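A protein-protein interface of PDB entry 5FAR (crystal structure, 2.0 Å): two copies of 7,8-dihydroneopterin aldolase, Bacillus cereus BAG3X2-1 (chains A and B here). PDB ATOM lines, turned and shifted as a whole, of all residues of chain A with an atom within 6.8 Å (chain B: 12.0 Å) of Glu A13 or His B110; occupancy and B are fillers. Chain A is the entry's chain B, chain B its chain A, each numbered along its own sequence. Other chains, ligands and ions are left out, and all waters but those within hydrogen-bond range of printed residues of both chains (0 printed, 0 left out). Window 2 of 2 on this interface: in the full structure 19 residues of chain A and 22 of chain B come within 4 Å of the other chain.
Of the printed residues of chain B, His A10 touches Tyr B111, Arg B112 and Ala B113. No residue of chain B comes within 4 Å of Phe A14. No residue of chain B comes within 4 Å of Arg A30. Pro B105 touches none of the printed residues of chain A. Of the printed residues of chain A, Pro B108 touches Phe A60. Of the printed residues of chain A, Arg B112 touches His A10 (2.8 Å) and Asp A11 (3.5 Å). The nearest residue of chain B that does not touch Glu A13 is Tyr B111 (4.5 Å). The nearest residue of chain A that does not touch His B110 is Phe A60 (4.1 Å). The nearest printed residue of chain A that does not touch Gly B109 is Glu A13 (5.9 Å).
Position printed for both chains: 103.
The backbone NH of Glu A13 is in hydrogen-bond range of the backbone carbonyl oxygen of His B110, 2.7 Å away. N of Arg B112 sits at hydrogen-bond distance from O of His A10 (2.8 Å). The backbone carbonyl oxygen of Ala B113 is in hydrogen-bond range of the backbone NH of His A10, 2.7 Å away.
O of Pro B105 lies within hydrogen-bond range of OH of Tyr B111 (2.7 Å). The side-chain hydroxyl of Tyr B111 lies within hydrogen-bond range of the backbone carbonyl oxygen of Ile B107 (2.9 Å). The side-chain amino group (NZ) of Lys A32 is in salt-bridge range of the side-chain carboxylate (OD1) of Asp A11, 3.6 Å away. N of Val A33 lies within hydrogen-bond range of O of Met A12, at 2.8 Å.
Among the printed residues, no Asp or Glu carboxylate lies within 4 Å of a Lys or Arg side-chain nitrogen of the other chain.
Tyr B111 touches His A10 (C to O, 3.8 Å). O of Asp A11 touches CA of Tyr B111, 3.3 Å away. Asp A11 touches Arg B112. O of His B110 touches CA of Met A12, at 3.3 Å. CA of Met A12 touches CA of Tyr B111, at 3.9 Å. CG2 of Ile B107 touches CD2 of Phe A60, 3.5 Å away. Phe A60 touches Pro B108 (CE2 to O, 3.4 Å). CA of Gly B109 touches CZ of Phe A60 (3.6 Å).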
ATOM      1  N   HIS A  10      26.744  10.855 -14.683  1.00  0.00           N
ATOM      2  CA  HIS A  10      25.406  10.354 -14.962  1.00  0.00           C
ATOM      3  C   HIS A  10      24.484  10.575 -13.781  1.00  0.00           C
ATOM      4  O   HIS A  10      24.792  10.138 -12.669  1.00  0.00           O
ATOM      5  CB  HIS A  10      25.444   8.845 -15.218  1.00  0.00           C
ATOM      6  CG  HIS A  10      26.166   8.457 -16.467  1.00  0.00           C
ATOM      7  ND1 HIS A  10      25.928   9.060 -17.686  1.00  0.00           N
ATOM      8  CD2 HIS A  10      27.108   7.513 -16.690  1.00  0.00           C
ATOM      9  CE1 HIS A  10      26.692   8.500 -18.606  1.00  0.00           C
ATOM     10  NE2 HIS A  10      27.423   7.566 -18.025  1.00  0.00           N
ATOM     11  N   ASP A  11      23.381  11.274 -14.029  1.00  0.00           N
ATOM     12  CA  ASP A  11      22.226  11.313 -13.133  1.00  0.00           C
ATOM     13  C   ASP A  11      22.536  11.933 -11.772  1.00  0.00           C
ATOM     14  O   ASP A  11      22.171  11.381 -10.735  1.00  0.00           O
ATOM     15  CB  ASP A  11      21.638   9.889 -12.987  1.00  0.00           C
ATOM     16  CG  ASP A  11      20.148   9.882 -12.647  1.00  0.00           C
ATOM     17  OD1 ASP A  11      19.514  10.953 -12.551  1.00  0.00           O
ATOM     18  OD2 ASP A  11      19.600   8.774 -12.498  1.00  0.00           O
ATOM     19  N   MET A  12      23.207  13.088 -11.787  1.00  0.00           N
ATOM     20  CA  MET A  12      23.416  13.889 -10.580  1.00  0.00           C
ATOM     21  C   MET A  12      22.049  14.281 -10.111  1.00  0.00           C
ATOM     22  O   MET A  12      21.212  14.660 -10.929  1.00  0.00           O
ATOM     23  CB  MET A  12      24.186  15.179 -10.842  1.00  0.00           C
ATOM     24  CG  MET A  12      25.682  14.894 -10.931  1.00  0.00           C
ATOM     25  SD  MET A  12      26.686  16.374 -11.783  1.00  0.00           S
ATOM     26  CE  MET A  12      25.922  16.163 -13.571  1.00  0.00           C
ATOM     27  N   GLU A  13      21.795  14.137  -8.812  1.00  0.00           N
ATOM     28  CA  GLU A  13      20.508  14.485  -8.228  1.00  0.00           C
ATOM     29  C   GLU A  13      20.706  15.590  -7.196  1.00  0.00           C
ATOM     30  O   GLU A  13      21.551  15.483  -6.326  1.00  0.00           O
ATOM     31  CB  GLU A  13      19.860  13.263  -7.553  1.00  0.00           C
ATOM     32  CG  GLU A  13      18.424  13.531  -7.137  1.00  0.00           C
ATOM     33  CD  GLU A  13      17.817  12.401  -6.336  1.00  0.00           C
ATOM     34  OE1 GLU A  13      18.185  12.256  -5.170  1.00  0.00           O
ATOM     35  OE2 GLU A  13      16.958  11.683  -6.852  1.00  0.00           O
ATOM     36  N   PHE A  14      19.885  16.632  -7.308  1.00  0.00           N
ATOM     37  CA  PHE A  14      19.907  17.785  -6.431  1.00  0.00           C
ATOM     38  C   PHE A  14      18.518  18.064  -5.961  1.00  0.00           C
ATOM     39  O   PHE A  14      17.549  17.537  -6.500  1.00  0.00           O
ATOM     40  CB  PHE A  14      20.399  19.014  -7.183  1.00  0.00           C
ATOM     41  CG  PHE A  14      21.756  18.835  -7.760  1.00  0.00           C
ATOM     42  CD1 PHE A  14      22.844  18.653  -6.916  1.00  0.00           C
ATOM     43  CD2 PHE A  14      21.951  18.799  -9.142  1.00  0.00           C
ATOM     44  CE1 PHE A  14      24.115  18.467  -7.438  1.00  0.00           C
ATOM     45  CE2 PHE A  14      23.217  18.612  -9.662  1.00  0.00           C
ATOM     46  CZ  PHE A  14      24.298  18.442  -8.821  1.00  0.00           C
ATOM     47  N   TYR A  15      18.434  18.889  -4.942  1.00  0.00           N
ATOM     48  CA  TYR A  15      17.196  19.523  -4.560  1.00  0.00           C
ATOM     49  C   TYR A  15      17.419  20.988  -4.841  1.00  0.00           C
ATOM     50  O   TYR A  15      18.414  21.540  -4.405  1.00  0.00           O
ATOM     51  CB  TYR A  15      16.887  19.296  -3.067  1.00  0.00           C
ATOM     52  CG  TYR A  15      15.426  19.478  -2.763  1.00  0.00           C
ATOM     53  CD1 TYR A  15      14.524  18.430  -2.947  1.00  0.00           C
ATOM     54  CD2 TYR A  15      14.934  20.705  -2.316  1.00  0.00           C
ATOM     55  CE1 TYR A  15      13.173  18.598  -2.681  1.00  0.00           C
ATOM     56  CE2 TYR A  15      13.576  20.888  -2.044  1.00  0.00           C
ATOM     57  CZ  TYR A  15      12.705  19.836  -2.228  1.00  0.00           C
ATOM     58  OH  TYR A  15      11.363  20.023  -1.978  1.00  0.00           O
ATOM     59  N   ARG A  30      13.041  17.965  -6.692  1.00  0.00           N
ATOM     60  CA  ARG A  30      14.219  17.262  -7.173  1.00  0.00           C
ATOM     61  C   ARG A  30      14.610  17.875  -8.518  1.00  0.00           C
ATOM     62  O   ARG A  30      13.737  18.223  -9.296  1.00  0.00           O
ATOM     63  CB  ARG A  30      13.945  15.786  -7.397  1.00  0.00           C
ATOM     64  CG  ARG A  30      13.690  14.937  -6.164  1.00  0.00           C
ATOM     65  CD  ARG A  30      13.580  13.502  -6.611  1.00  0.00           C
ATOM     66  NE  ARG A  30      13.104  12.587  -5.578  1.00  0.00           N
ATOM     67  CZ  ARG A  30      11.852  12.152  -5.407  1.00  0.00           C
ATOM     68  NH1 ARG A  30      10.836  12.531  -6.189  1.00  0.00           N
ATOM     69  NH2 ARG A  30      11.608  11.303  -4.398  1.00  0.00           N
ATOM     70  N   PHE A  31      15.911  18.014  -8.751  1.00  0.00           N
ATOM     71  CA  PHE A  31      16.466  18.298 -10.074  1.00  0.00           C
ATOM     72  C   PHE A  31      17.567  17.291 -10.324  1.00  0.00           C
ATOM     73  O   PHE A  31      18.323  16.950  -9.409  1.00  0.00           O
ATOM     74  CB  PHE A  31      17.017  19.725 -10.155  1.00  0.00           C
ATOM     75  CG  PHE A  31      15.954  20.765 -10.214  1.00  0.00           C
ATOM     76  CD1 PHE A  31      15.353  21.211  -9.052  1.00  0.00           C
ATOM     77  CD2 PHE A  31      15.528  21.280 -11.435  1.00  0.00           C
ATOM     78  CE1 PHE A  31      14.350  22.161  -9.098  1.00  0.00           C
ATOM     79  CE2 PHE A  31      14.524  22.235 -11.486  1.00  0.00           C
ATOM     80  CZ  PHE A  31      13.940  22.680 -10.313  1.00  0.00           C
ATOM     81  N   LYS A  32      17.631  16.801 -11.554  1.00  0.00           N
ATOM     82  CA  LYS A  32      18.662  15.887 -12.000  1.00  0.00           C
ATOM     83  C   LYS A  32      19.457  16.527 -13.131  1.00  0.00           C
ATOM     84  O   LYS A  32      18.927  17.374 -13.853  1.00  0.00           O
ATOM     85  CB  LYS A  32      18.035  14.588 -12.489  1.00  0.00           C
ATOM     86  CG  LYS A  32      17.559  13.666 -11.382  1.00  0.00           C
ATOM     87  CD  LYS A  32      16.585  12.658 -11.965  1.00  0.00           C
ATOM     88  CE  LYS A  32      16.554  11.349 -11.204  1.00  0.00           C
ATOM     89  NZ  LYS A  32      16.048  10.289 -12.101  1.00  0.00           N
ATOM     90  N   VAL A  33      20.728  16.154 -13.255  1.00  0.00           N
ATOM     91  CA  VAL A  33      21.590  16.673 -14.325  1.00  0.00           C
ATOM     92  C   VAL A  33      22.511  15.567 -14.836  1.00  0.00           C
ATOM     93  O   VAL A  33      23.173  14.894 -14.035  1.00  0.00           O
ATOM     94  CB  VAL A  33      22.429  17.898 -13.873  1.00  0.00           C
ATOM     95  CG1 VAL A  33      23.254  18.472 -15.038  1.00  0.00           C
ATOM     96  CG2 VAL A  33      21.547  18.998 -13.292  1.00  0.00           C
ATOM     97  N   PHE A  60      31.358  17.757 -10.924  1.00  0.00           N
ATOM     98  CA  PHE A  60      30.169  17.579 -10.081  1.00  0.00           C
ATOM     99  C   PHE A  60      29.910  18.844  -9.308  1.00  0.00           C
ATOM    100  O   PHE A  60      28.836  19.439  -9.402  1.00  0.00           O
ATOM    101  CB  PHE A  60      30.310  16.416  -9.089  1.00  0.00           C
ATOM    102  CG  PHE A  60      29.234  16.405  -8.027  1.00  0.00           C
ATOM    103  CD1 PHE A  60      27.997  15.858  -8.302  1.00  0.00           C
ATOM    104  CD2 PHE A  60      29.449  16.971  -6.775  1.00  0.00           C
ATOM    105  CE1 PHE A  60      26.987  15.837  -7.349  1.00  0.00           C
ATOM    106  CE2 PHE A  60      28.444  16.953  -5.806  1.00  0.00           C
ATOM    107  CZ  PHE A  60      27.205  16.400  -6.102  1.00  0.00           C
ATOM    108  N   VAL A  67      22.991  24.439  -9.530  1.00  0.00           N
ATOM    109  CA  VAL A  67      21.666  23.926  -9.172  1.00  0.00           C
ATOM    110  C   VAL A  67      21.251  24.270  -7.717  1.00  0.00           C
ATOM    111  O   VAL A  67      20.068  24.551  -7.463  1.00  0.00           O
ATOM    112  CB  VAL A  67      21.559  22.395  -9.422  1.00  0.00           C
ATOM    113  CG1 VAL A  67      20.144  21.907  -9.137  1.00  0.00           C
ATOM    114  CG2 VAL A  67      21.940  22.048 -10.866  1.00  0.00           C
ATOM    115  N   GLU A  68      22.202  24.248  -6.780  1.00  0.00           N
ATOM    116  CA  GLU A  68      21.918  24.492  -5.342  1.00  0.00           C
ATOM    117  C   GLU A  68      22.126  25.954  -4.903  1.00  0.00           C
ATOM    118  O   GLU A  68      21.217  26.579  -4.358  1.00  0.00           O
ATOM    119  CB  GLU A  68      22.768  23.564  -4.460  1.00  0.00           C
ATOM    120  CG  GLU A  68      22.530  22.073  -4.685  1.00  0.00           C
ATOM    121  CD  GLU A  68      23.051  21.185  -3.555  1.00  0.00           C
ATOM    122  OE1 GLU A  68      23.840  21.641  -2.694  1.00  0.00           O
ATOM    123  OE2 GLU A  68      22.702  20.000  -3.546  1.00  0.00           O
ATOM    124  N   PRO A 103      12.073  15.821 -12.735  1.00  0.00           N
ATOM    125  CA  PRO A 103      11.343  14.542 -12.675  1.00  0.00           C
ATOM    126  C   PRO A 103       9.932  14.644 -12.067  1.00  0.00           C
ATOM    127  O   PRO A 103       9.076  13.797 -12.338  1.00  0.00           O
ATOM    128  CB  PRO A 103      12.262  13.682 -11.802  1.00  0.00           C
ATOM    129  CG  PRO A 103      12.877  14.668 -10.866  1.00  0.00           C
ATOM    130  CD  PRO A 103      13.158  15.861 -11.741  1.00  0.00           C
ATOM    131  N   LYS B 102      32.911   4.358 -13.271  1.00  0.00           N
ATOM    132  CA  LYS B 102      33.229   4.330 -11.851  1.00  0.00           C
ATOM    133  C   LYS B 102      31.897   4.655 -11.148  1.00  0.00           C
ATOM    134  O   LYS B 102      31.548   5.813 -11.031  1.00  0.00           O
ATOM    135  CB  LYS B 102      34.319   5.385 -11.561  1.00  0.00           C
ATOM    136  CG  LYS B 102      35.430   4.970 -10.609  1.00  0.00           C
ATOM    137  CD  LYS B 102      36.339   6.145 -10.249  1.00  0.00           C
ATOM    138  CE  LYS B 102      37.765   5.694  -9.956  1.00  0.00           C
ATOM    139  NZ  LYS B 102      38.560   6.662  -9.152  1.00  0.00           N
ATOM    140  N   PRO B 103      31.105   3.637 -10.744  1.00  0.00           N
ATOM    141  CA  PRO B 103      29.793   3.933 -10.096  1.00  0.00           C
ATOM    142  C   PRO B 103      29.818   4.512  -8.671  1.00  0.00           C
ATOM    143  O   PRO B 103      28.849   5.180  -8.258  1.00  0.00           O
ATOM    144  CB  PRO B 103      29.103   2.568 -10.079  1.00  0.00           C
ATOM    145  CG  PRO B 103      30.227   1.589 -10.049  1.00  0.00           C
ATOM    146  CD  PRO B 103      31.283   2.195 -10.950  1.00  0.00           C
ATOM    147  N   ASP B 104      30.877   4.223  -7.921  1.00  0.00           N
ATOM    148  CA  ASP B 104      30.995   4.597  -6.506  1.00  0.00           C
ATOM    149  C   ASP B 104      32.291   5.338  -6.263  1.00  0.00           C
ATOM    150  O   ASP B 104      33.112   4.894  -5.460  1.00  0.00           O
ATOM    151  CB  ASP B 104      30.920   3.334  -5.621  1.00  0.00           C
ATOM    152  CG  ASP B 104      29.926   2.330  -6.144  1.00  0.00           C
ATOM    153  OD1 ASP B 104      28.826   2.755  -6.519  1.00  0.00           O
ATOM    154  OD2 ASP B 104      30.241   1.128  -6.221  1.00  0.00           O
ATOM    155  N   PRO B 105      32.481   6.494  -6.940  1.00  0.00           N
ATOM    156  CA  PRO B 105      33.625   7.332  -6.662  1.00  0.00           C
ATOM    157  C   PRO B 105      33.467   8.116  -5.369  1.00  0.00           C
ATOM    158  O   PRO B 105      32.345   8.396  -4.953  1.00  0.00           O
ATOM    159  CB  PRO B 105      33.626   8.319  -7.837  1.00  0.00           C
ATOM    160  CG  PRO B 105      32.191   8.497  -8.129  1.00  0.00           C
ATOM    161  CD  PRO B 105      31.600   7.124  -7.935  1.00  0.00           C
ATOM    162  N   PRO B 106      34.581   8.551  -4.777  1.00  0.00           N
ATOM    163  CA  PRO B 106      34.485   9.334  -3.555  1.00  0.00           C
ATOM    164  C   PRO B 106      34.155  10.826  -3.772  1.00  0.00           C
ATOM    165  O   PRO B 106      34.915  11.687  -3.349  1.00  0.00           O
ATOM    166  CB  PRO B 106      35.860   9.124  -2.922  1.00  0.00           C
ATOM    167  CG  PRO B 106      36.771   8.963  -4.094  1.00  0.00           C
ATOM    168  CD  PRO B 106      35.967   8.150  -5.072  1.00  0.00           C
ATOM    169  N   ILE B 107      33.028  11.122  -4.430  1.00  0.00           N
ATOM    170  CA  ILE B 107      32.515  12.481  -4.498  1.00  0.00           C
ATOM    171  C   ILE B 107      31.407  12.594  -3.457  1.00  0.00           C
ATOM    172  O   ILE B 107      30.462  11.786  -3.465  1.00  0.00           O
ATOM    173  CB  ILE B 107      31.962  12.859  -5.882  1.00  0.00           C
ATOM    174  CG1 ILE B 107      32.994  12.565  -6.979  1.00  0.00           C
ATOM    175  CG2 ILE B 107      31.619  14.344  -5.913  1.00  0.00           C
ATOM    176  CD1 ILE B 107      32.374  12.478  -8.355  1.00  0.00           C
ATOM    177  N   PRO B 108      31.538  13.555  -2.529  1.00  0.00           N
ATOM    178  CA  PRO B 108      30.395  13.851  -1.657  1.00  0.00           C
ATOM    179  C   PRO B 108      29.209  14.396  -2.451  1.00  0.00           C
ATOM    180  O   PRO B 108      29.224  15.533  -2.853  1.00  0.00           O
ATOM    181  CB  PRO B 108      30.952  14.893  -0.673  1.00  0.00           C
ATOM    182  CG  PRO B 108      32.407  14.643  -0.658  1.00  0.00           C
ATOM    183  CD  PRO B 108      32.745  14.277  -2.084  1.00  0.00           C
ATOM    184  N   GLY B 109      28.213  13.549  -2.702  1.00  0.00           N
ATOM    185  CA  GLY B 109      27.042  13.957  -3.462  1.00  0.00           C
ATOM    186  C   GLY B 109      26.284  12.787  -4.041  1.00  0.00           C
ATOM    187  O   GLY B 109      26.668  11.620  -3.871  1.00  0.00           O
ATOM    188  N   HIS B 110      25.211  13.120  -4.753  1.00  0.00           N
ATOM    189  CA  HIS B 110      24.250  12.157  -5.219  1.00  0.00           C
ATOM    190  C   HIS B 110      24.200  12.114  -6.735  1.00  0.00           C
ATOM    191  O   HIS B 110      23.828  13.080  -7.363  1.00  0.00           O
ATOM    192  CB  HIS B 110      22.904  12.511  -4.613  1.00  0.00           C
ATOM    193  CG  HIS B 110      23.001  12.806  -3.157  1.00  0.00           C
ATOM    194  ND1 HIS B 110      22.869  11.832  -2.190  1.00  0.00           N
ATOM    195  CD2 HIS B 110      23.323  13.944  -2.503  1.00  0.00           C
ATOM    196  CE1 HIS B 110      23.067  12.370  -1.000  1.00  0.00           C
ATOM    197  NE2 HIS B 110      23.347  13.649  -1.167  1.00  0.00           N
ATOM    198  N   TYR B 111      24.588  10.969  -7.290  1.00  0.00           N
ATOM    199  CA  TYR B 111      24.738  10.759  -8.737  1.00  0.00           C
ATOM    200  C   TYR B 111      24.580   9.267  -8.977  1.00  0.00           C
ATOM    201  O   TYR B 111      24.512   8.513  -8.014  1.00  0.00           O
ATOM    202  CB  TYR B 111      26.131  11.243  -9.208  1.00  0.00           C
ATOM    203  CG  TYR B 111      27.217  10.844  -8.248  1.00  0.00           C
ATOM    204  CD1 TYR B 111      27.775   9.571  -8.283  1.00  0.00           C
ATOM    205  CD2 TYR B 111      27.658  11.727  -7.264  1.00  0.00           C
ATOM    206  CE1 TYR B 111      28.723   9.194  -7.357  1.00  0.00           C
ATOM    207  CE2 TYR B 111      28.612  11.358  -6.337  1.00  0.00           C
ATOM    208  CZ  TYR B 111      29.139  10.097  -6.389  1.00  0.00           C
ATOM    209  OH  TYR B 111      30.100   9.750  -5.477  1.00  0.00           O
ATOM    210  N   ARG B 112      24.549   8.826 -10.240  1.00  0.00           N
ATOM    211  CA  ARG B 112      24.617   7.395 -10.540  1.00  0.00           C
ATOM    212  C   ARG B 112      26.044   6.933 -10.737  1.00  0.00           C
ATOM    213  O   ARG B 112      26.420   5.885 -10.206  1.00  0.00           O
ATOM    214  CB  ARG B 112      23.775   7.014 -11.765  1.00  0.00           C
ATOM    215  CG  ARG B 112      23.890   5.535 -12.145  1.00  0.00           C
ATOM    216  CD  ARG B 112      22.710   5.045 -12.971  1.00  0.00           C
ATOM    217  NE  ARG B 112      22.432   5.903 -14.124  1.00  0.00           N
ATOM    218  CZ  ARG B 112      23.151   5.947 -15.253  1.00  0.00           C
ATOM    219  NH1 ARG B 112      24.234   5.180 -15.435  1.00  0.00           N
ATOM    220  NH2 ARG B 112      22.776   6.778 -16.225  1.00  0.00           N
ATOM    221  N   ALA B 113      26.830   7.681 -11.525  1.00  0.00           N
ATOM    222  CA  ALA B 113      28.166   7.253 -11.892  1.00  0.00           C
ATOM    223  C   ALA B 113      28.923   8.369 -12.623  1.00  0.00           C
ATOM    224  O   ALA B 113      28.306   9.268 -13.207  1.00  0.00           O
ATOM    225  CB  ALA B 113      28.089   6.015 -12.776  1.00  0.00           C
ATOM    226  N   VAL B 114      30.253   8.312 -12.562  1.00  0.00           N
ATOM    227  CA  VAL B 114      31.113   9.083 -13.474  1.00  0.00           C
ATOM    228  C   VAL B 114      31.702   8.084 -14.450  1.00  0.00           C
ATOM    229  O   VAL B 114      31.659   6.866 -14.192  1.00  0.00           O
ATOM    230  CB  VAL B 114      32.202   9.905 -12.736  1.00  0.00           C
ATOM    231  CG1 VAL B 114      31.579  10.668 -11.581  1.00  0.00           C
ATOM    232  CG2 VAL B 114      33.351   9.039 -12.236  1.00  0.00           C
